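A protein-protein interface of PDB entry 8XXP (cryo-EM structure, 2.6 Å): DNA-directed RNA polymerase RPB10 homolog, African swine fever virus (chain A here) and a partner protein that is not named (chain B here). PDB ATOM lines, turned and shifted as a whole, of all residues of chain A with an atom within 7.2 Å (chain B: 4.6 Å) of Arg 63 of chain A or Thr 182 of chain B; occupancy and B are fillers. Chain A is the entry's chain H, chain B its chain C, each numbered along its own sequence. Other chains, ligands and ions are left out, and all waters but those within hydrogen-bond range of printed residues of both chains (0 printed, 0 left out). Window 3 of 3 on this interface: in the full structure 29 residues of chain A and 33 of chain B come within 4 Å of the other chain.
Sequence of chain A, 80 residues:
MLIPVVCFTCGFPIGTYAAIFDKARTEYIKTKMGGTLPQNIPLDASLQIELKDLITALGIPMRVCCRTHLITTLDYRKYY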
ATOM      1  N   CYS A   7       2.476 -11.482  11.489  1.00  0.00           N
ATOM      2  CA  CYS A   7       3.285 -12.180  10.501  1.00  0.00           C
ATOM      3  C   CYS A   7       2.781 -11.859   9.102  1.00  0.00           C
ATOM      4  O   CYS A   7       1.579 -11.906   8.837  1.00  0.00           O
ATOM      5  CB  CYS A   7       3.238 -13.683  10.757  1.00  0.00           C
ATOM      6  SG  CYS A   7       3.914 -14.708   9.451  1.00  0.00           S
ATOM      7  N   THR A   9       2.964 -13.587   6.526  1.00  0.00           N
ATOM      8  CA  THR A   9       2.515 -14.776   5.822  1.00  0.00           C
ATOM      9  C   THR A   9       1.189 -15.308   6.347  1.00  0.00           C
ATOM     10  O   THR A   9       0.263 -15.542   5.567  1.00  0.00           O
ATOM     11  CB  THR A   9       3.593 -15.852   5.915  1.00  0.00           C
ATOM     12  OG1 THR A   9       4.831 -15.325   5.431  1.00  0.00           O
ATOM     13  CG2 THR A   9       3.221 -17.047   5.106  1.00  0.00           C
ATOM     14  N   CYS A  10       1.072 -15.502   7.658  1.00  0.00           N
ATOM     15  CA  CYS A  10      -0.109 -16.122   8.234  1.00  0.00           C
ATOM     16  C   CYS A  10      -0.968 -15.182   9.063  1.00  0.00           C
ATOM     17  O   CYS A  10      -2.131 -15.506   9.317  1.00  0.00           O
ATOM     18  CB  CYS A  10       0.293 -17.315   9.105  1.00  0.00           C
ATOM     19  SG  CYS A  10       0.954 -16.852  10.693  1.00  0.00           S
ATOM     20  N   GLY A  11      -0.444 -14.041   9.488  1.00  0.00           N
ATOM     21  CA  GLY A  11      -1.226 -13.108  10.262  1.00  0.00           C
ATOM     22  C   GLY A  11      -1.211 -13.325  11.754  1.00  0.00           C
ATOM     23  O   GLY A  11      -2.003 -12.696  12.459  1.00  0.00           O
ATOM     24  N   PHE A  12      -0.360 -14.205  12.254  1.00  0.00           N
ATOM     25  CA  PHE A  12      -0.193 -14.331  13.689  1.00  0.00           C
ATOM     26  C   PHE A  12       0.445 -13.061  14.245  1.00  0.00           C
ATOM     27  O   PHE A  12       1.386 -12.531  13.651  1.00  0.00           O
ATOM     28  CB  PHE A  12       0.667 -15.547  14.020  1.00  0.00           C
ATOM     29  CG  PHE A  12       0.798 -15.810  15.483  1.00  0.00           C
ATOM     30  CD1 PHE A  12      -0.160 -16.537  16.153  1.00  0.00           C
ATOM     31  CD2 PHE A  12       1.880 -15.327  16.190  1.00  0.00           C
ATOM     32  CE1 PHE A  12      -0.043 -16.774  17.492  1.00  0.00           C
ATOM     33  CE2 PHE A  12       2.000 -15.559  17.530  1.00  0.00           C
ATOM     34  CZ  PHE A  12       1.039 -16.284  18.184  1.00  0.00           C
ATOM     35  N   ILE A  60       5.376 -17.432  20.794  1.00  0.00           N
ATOM     36  CA  ILE A  60       5.296 -17.610  19.342  1.00  0.00           C
ATOM     37  C   ILE A  60       5.536 -19.078  19.009  1.00  0.00           C
ATOM     38  O   ILE A  60       6.555 -19.647  19.435  1.00  0.00           O
ATOM     39  CB  ILE A  60       6.305 -16.709  18.634  1.00  0.00           C
ATOM     40  CG1 ILE A  60       5.901 -15.245  18.770  1.00  0.00           C
ATOM     41  CG2 ILE A  60       6.410 -17.071  17.171  1.00  0.00           C
ATOM     42  CD1 ILE A  60       6.894 -14.414  19.512  1.00  0.00           C
ATOM     43  N   PRO A  61       4.640 -19.729  18.276  1.00  0.00           N
ATOM     44  CA  PRO A  61       4.792 -21.169  18.030  1.00  0.00           C
ATOM     45  C   PRO A  61       5.890 -21.493  17.030  1.00  0.00           C
ATOM     46  O   PRO A  61       6.484 -20.594  16.435  1.00  0.00           O
ATOM     47  CB  PRO A  61       3.414 -21.574  17.499  1.00  0.00           C
ATOM     48  CG  PRO A  61       2.877 -20.328  16.885  1.00  0.00           C
ATOM     49  CD  PRO A  61       3.406 -19.187  17.683  1.00  0.00           C
ATOM     50  N   MET A  62       6.158 -22.783  16.837  1.00  0.00           N
ATOM     51  CA  MET A  62       7.144 -23.240  15.865  1.00  0.00           C
ATOM     52  C   MET A  62       6.623 -23.081  14.445  1.00  0.00           C
ATOM     53  O   MET A  62       6.417 -24.073  13.741  1.00  0.00           O
ATOM     54  CB  MET A  62       7.503 -24.704  16.113  1.00  0.00           C
ATOM     55  CG  MET A  62       8.670 -24.953  17.032  1.00  0.00           C
ATOM     56  SD  MET A  62      10.212 -24.298  16.385  1.00  0.00           S
ATOM     57  CE  MET A  62      10.812 -23.437  17.819  1.00  0.00           C
ATOM     58  N   ARG A  63       6.411 -21.846  14.015  1.00  0.00           N
ATOM     59  CA  ARG A  63       5.944 -21.553  12.671  1.00  0.00           C
ATOM     60  C   ARG A  63       7.094 -20.967  11.875  1.00  0.00           C
ATOM     61  O   ARG A  63       7.730 -20.009  12.317  1.00  0.00           O
ATOM     62  CB  ARG A  63       4.762 -20.586  12.702  1.00  0.00           C
ATOM     63  CG  ARG A  63       3.512 -21.164  13.320  1.00  0.00           C
ATOM     64  CD  ARG A  63       2.402 -20.137  13.382  1.00  0.00           C
ATOM     65  NE  ARG A  63       1.740 -19.950  12.099  1.00  0.00           N
ATOM     66  CZ  ARG A  63       0.830 -20.768  11.597  1.00  0.00           C
ATOM     67  NH1 ARG A  63       0.447 -21.854  12.242  1.00  0.00           N
ATOM     68  NH2 ARG A  63       0.289 -20.491  10.416  1.00  0.00           N
ATOM     69  N   VAL A  64       7.363 -21.547  10.706  1.00  0.00           N
ATOM     70  CA  VAL A  64       8.486 -21.095   9.891  1.00  0.00           C
ATOM     71  C   VAL A  64       8.309 -19.633   9.516  1.00  0.00           C
ATOM     72  O   VAL A  64       9.268 -18.856   9.515  1.00  0.00           O
ATOM     73  CB  VAL A  64       8.630 -21.990   8.646  1.00  0.00           C
ATOM     74  CG1 VAL A  64       9.608 -21.387   7.658  1.00  0.00           C
ATOM     75  CG2 VAL A  64       9.074 -23.374   9.047  1.00  0.00           C
ATOM     76  N   CYS A  65       7.078 -19.232   9.213  1.00  0.00           N
ATOM     77  CA  CYS A  65       6.828 -17.868   8.765  1.00  0.00           C
ATOM     78  C   CYS A  65       6.981 -16.870   9.903  1.00  0.00           C
ATOM     79  O   CYS A  65       7.585 -15.808   9.731  1.00  0.00           O
ATOM     80  CB  CYS A  65       5.435 -17.781   8.151  1.00  0.00           C
ATOM     81  SG  CYS A  65       4.116 -18.458   9.173  1.00  0.00           S
ATOM     82  N   CYS A  66       6.435 -17.190  11.075  1.00  0.00           N
ATOM     83  CA  CYS A  66       6.410 -16.227  12.168  1.00  0.00           C
ATOM     84  C   CYS A  66       7.800 -15.976  12.726  1.00  0.00           C
ATOM     85  O   CYS A  66       8.146 -14.835  13.046  1.00  0.00           O
ATOM     86  CB  CYS A  66       5.471 -16.713  13.263  1.00  0.00           C
ATOM     87  SG  CYS A  66       3.806 -16.946  12.691  1.00  0.00           S
ATOM     88  N   ARG A  67       8.600 -17.025  12.871  1.00  0.00           N
ATOM     89  CA  ARG A  67       9.962 -16.871  13.355  1.00  0.00           C
ATOM     90  C   ARG A  67      10.893 -16.304  12.300  1.00  0.00           C
ATOM     91  O   ARG A  67      11.920 -15.718  12.652  1.00  0.00           O
ATOM     92  CB  ARG A  67      10.483 -18.213  13.845  1.00  0.00           C
ATOM     93  CG  ARG A  67       9.478 -18.907  14.702  1.00  0.00           C
ATOM     94  CD  ARG A  67      10.121 -19.797  15.713  1.00  0.00           C
ATOM     95  NE  ARG A  67       9.155 -20.169  16.734  1.00  0.00           N
ATOM     96  CZ  ARG A  67       9.468 -20.413  17.994  1.00  0.00           C
ATOM     97  NH1 ARG A  67      10.717 -20.343  18.418  1.00  0.00           N
ATOM     98  NH2 ARG A  67       8.506 -20.743  18.849  1.00  0.00           N
ATOM     99  N   THR A  68      10.563 -16.467  11.023  1.00  0.00           N
ATOM    100  CA  THR A  68      11.346 -15.837   9.969  1.00  0.00           C
ATOM    101  C   THR A  68      11.218 -14.321  10.024  1.00  0.00           C
ATOM    102  O   THR A  68      12.221 -13.603  10.015  1.00  0.00           O
ATOM    103  CB  THR A  68      10.898 -16.359   8.608  1.00  0.00           C
ATOM    104  OG1 THR A  68      11.326 -17.714   8.450  1.00  0.00           O
ATOM    105  CG2 THR A  68      11.482 -15.524   7.513  1.00  0.00           C
ATOM    106  N   HIS A  69       9.987 -13.817  10.088  1.00  0.00           N
ATOM    107  CA  HIS A  69       9.772 -12.378  10.075  1.00  0.00           C
ATOM    108  C   HIS A  69      10.127 -11.735  11.401  1.00  0.00           C
ATOM    109  O   HIS A  69      10.377 -10.528  11.444  1.00  0.00           O
ATOM    110  CB  HIS A  69       8.322 -12.074   9.710  1.00  0.00           C
ATOM    111  CG  HIS A  69       7.905 -12.646   8.393  1.00  0.00           C
ATOM    112  ND1 HIS A  69       8.604 -12.415   7.228  1.00  0.00           N
ATOM    113  CD2 HIS A  69       6.870 -13.447   8.057  1.00  0.00           C
ATOM    114  CE1 HIS A  69       8.016 -13.051   6.232  1.00  0.00           C
ATOM    115  NE2 HIS A  69       6.961 -13.683   6.708  1.00  0.00           N
ATOM    116  N   ASN B  42      -4.907 -21.478  20.734  1.00  0.00           N
ATOM    117  CA  ASN B  42      -4.881 -22.519  19.721  1.00  0.00           C
ATOM    118  C   ASN B  42      -5.976 -23.530  20.025  1.00  0.00           C
ATOM    119  O   ASN B  42      -5.950 -24.184  21.072  1.00  0.00           O
ATOM    120  CB  ASN B  42      -3.517 -23.201  19.684  1.00  0.00           C
ATOM    121  CG  ASN B  42      -3.421 -24.242  18.604  1.00  0.00           C
ATOM    122  OD1 ASN B  42      -3.985 -24.085  17.525  1.00  0.00           O
ATOM    123  ND2 ASN B  42      -2.706 -25.319  18.886  1.00  0.00           N
ATOM    124  N   VAL B 180      -5.865 -18.233  12.222  1.00  0.00           N
ATOM    125  CA  VAL B 180      -4.755 -18.758  11.445  1.00  0.00           C
ATOM    126  C   VAL B 180      -4.763 -20.270  11.587  1.00  0.00           C
ATOM    127  O   VAL B 180      -5.217 -20.821  12.594  1.00  0.00           O
ATOM    128  CB  VAL B 180      -3.402 -18.143  11.867  1.00  0.00           C
ATOM    129  CG1 VAL B 180      -3.608 -16.747  12.402  1.00  0.00           C
ATOM    130  CG2 VAL B 180      -2.681 -19.009  12.876  1.00  0.00           C
ATOM    131  N   LYS B 181      -4.288 -20.948  10.551  1.00  0.00           N
ATOM    132  CA  LYS B 181      -4.290 -22.401  10.508  1.00  0.00           C
ATOM    133  C   LYS B 181      -3.075 -22.937  11.245  1.00  0.00           C
ATOM    134  O   LYS B 181      -1.948 -22.518  10.979  1.00  0.00           O
ATOM    135  CB  LYS B 181      -4.277 -22.890   9.062  1.00  0.00           C
ATOM    136  CG  LYS B 181      -5.496 -22.499   8.265  1.00  0.00           C
ATOM    137  CD  LYS B 181      -5.322 -22.847   6.813  1.00  0.00           C
ATOM    138  CE  LYS B 181      -4.243 -22.004   6.176  1.00  0.00           C
ATOM    139  NZ  LYS B 181      -4.672 -20.603   5.970  1.00  0.00           N
ATOM    140  N   THR B 182      -3.305 -23.860  12.175  1.00  0.00           N
ATOM    141  CA  THR B 182      -2.212 -24.538  12.851  1.00  0.00           C
ATOM    142  C   THR B 182      -2.176 -26.036  12.614  1.00  0.00           C
ATOM    143  O   THR B 182      -1.122 -26.642  12.816  1.00  0.00           O
ATOM    144  CB  THR B 182      -2.255 -24.283  14.365  1.00  0.00           C
ATOM    145  OG1 THR B 182      -3.267 -25.093  14.971  1.00  0.00           O
ATOM    146  CG2 THR B 182      -2.525 -22.829  14.653  1.00  0.00           C
ATOM    147  N   HIS B 183      -3.278 -26.645  12.193  1.00  0.00           N
ATOM    148  CA  HIS B 183      -3.283 -28.075  11.940  1.00  0.00           C
ATOM    149  C   HIS B 183      -4.460 -28.439  11.054  1.00  0.00           C
ATOM    150  O   HIS B 183      -5.537 -27.850  11.152  1.00  0.00           O
ATOM    151  CB  HIS B 183      -3.344 -28.877  13.239  1.00  0.00           C
ATOM    152  CG  HIS B 183      -3.139 -30.341  13.040  1.00  0.00           C
ATOM    153  ND1 HIS B 183      -1.891 -30.922  13.034  1.00  0.00           N
ATOM    154  CD2 HIS B 183      -4.022 -31.341  12.819  1.00  0.00           C
ATOM    155  CE1 HIS B 183      -2.015 -32.219  12.826  1.00  0.00           C
ATOM    156  NE2 HIS B 183      -3.298 -32.498  12.693  1.00  0.00           N
ATOM    157  N   GLY B 220      -7.096 -27.580  13.453  1.00  0.00           N
ATOM    158  CA  GLY B 220      -6.464 -26.742  14.448  1.00  0.00           C
ATOM    159  C   GLY B 220      -6.346 -25.306  13.995  1.00  0.00           C
ATOM    160  O   GLY B 220      -5.631 -25.008  13.037  1.00  0.00           O
ATOM    161  N   LEU B 221      -7.047 -24.407  14.672  1.00  0.00           N
ATOM    162  CA  LEU B 221      -7.073 -22.996  14.319  1.00  0.00           C
ATOM    163  C   LEU B 221      -6.650 -22.169  15.517  1.00  0.00           C
ATOM    164  O   LEU B 221      -7.047 -22.456  16.647  1.00  0.00           O
ATOM    165  CB  LEU B 221      -8.465 -22.567  13.871  1.00  0.00           C
ATOM    166  CG  LEU B 221      -8.977 -23.159  12.566  1.00  0.00           C
ATOM    167  CD1 LEU B 221     -10.395 -22.707  12.329  1.00  0.00           C
ATOM    168  CD2 LEU B 221      -8.086 -22.746  11.418  1.00  0.00           C
ATOM    169  N   CYS B 222      -5.850 -21.140  15.271  1.00  0.00           N
ATOM    170  CA  CYS B 222      -5.403 -20.234  16.317  1.00  0.00           C
ATOM    171  C   CYS B 222      -6.132 -18.909  16.182  1.00  0.00           C
ATOM    172  O   CYS B 222      -6.213 -18.348  15.087  1.00  0.00           O
ATOM    173  CB  CYS B 222      -3.892 -20.010  16.253  1.00  0.00           C
ATOM    174  SG  CYS B 222      -3.279 -18.754  17.379  1.00  0.00           S
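The backbone carbonyl oxygen (O) of Lys 181 of chain B lies within hydrogen-bond range of the guanidinium group (NH1) of Arg 63 of chain A (2.8 Å).
The backbone carbonyl oxygen (O) of Phe 12 of chain A lies within hydrogen-bond range of the backbone NH (N) of Cys 7 of chain A, at 2.6 Å.
The backbone carbonyl oxygen (O) of Val 180 of chain B lies within hydrogen-bond range of the backbone NH (N) of Cys 222 of chain B (2.8 Å).
The side-chain sulfur (SG) of Cys 10 of chain A lies close to the guanidinium group (NE) of Arg 63 of chain A, 3.5 Å away.
The side-chain amide oxygen of Asn 42 of chain B sits at hydrogen-bond distance from the side-chain hydroxyl of Thr 182 of chain B, at 2.8 Å.
The backbone carbonyl oxygen (O) of Gly 220 of chain B sits at hydrogen-bond distance from the backbone NH (N) of Thr 182 of chain B (2.7 Å).
The side-chain sulfur (SG) of Cys 66 of chain A sits close to the guanidinium group (NE) of Arg 63 of chain A.
O of Cys 10 of chain A touches CG1 of Val 180 of chain B, 3.6 Å away.
Phe 12 of chain A touches Cys 222 of chain B (CE1 to SG, 3.8 Å).
Thr 182 of chain B touches Arg 63 of chain A.
Of the printed residues of chain B, Cys 10 of chain A touches Val 180.
Arg 63 of chain A touches just these residues of chain B: Lys 181 and Thr 182.
Of the printed residues of chain A, Lys 181 of chain B touches Arg 63 (2.8 Å).
Thr 182 of chain B touches one residue of chain A.
Printed residues of chain A within 4 Å of Cys 222 of chain B: Phe 12.
The nearest residue of chain A that does not touch Thr 182 of chain B is Pro 61 of chain A (6.4 Å).
Hydrophobic or aromatic side chains of chain B that line the printed part of chain A: Val 180.
Hydrophobic or aromatic side chains of chain A within 4 Å of the printed part of chain B: Phe 12.
Among the printed residues, 4 pairs touch across the chains.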
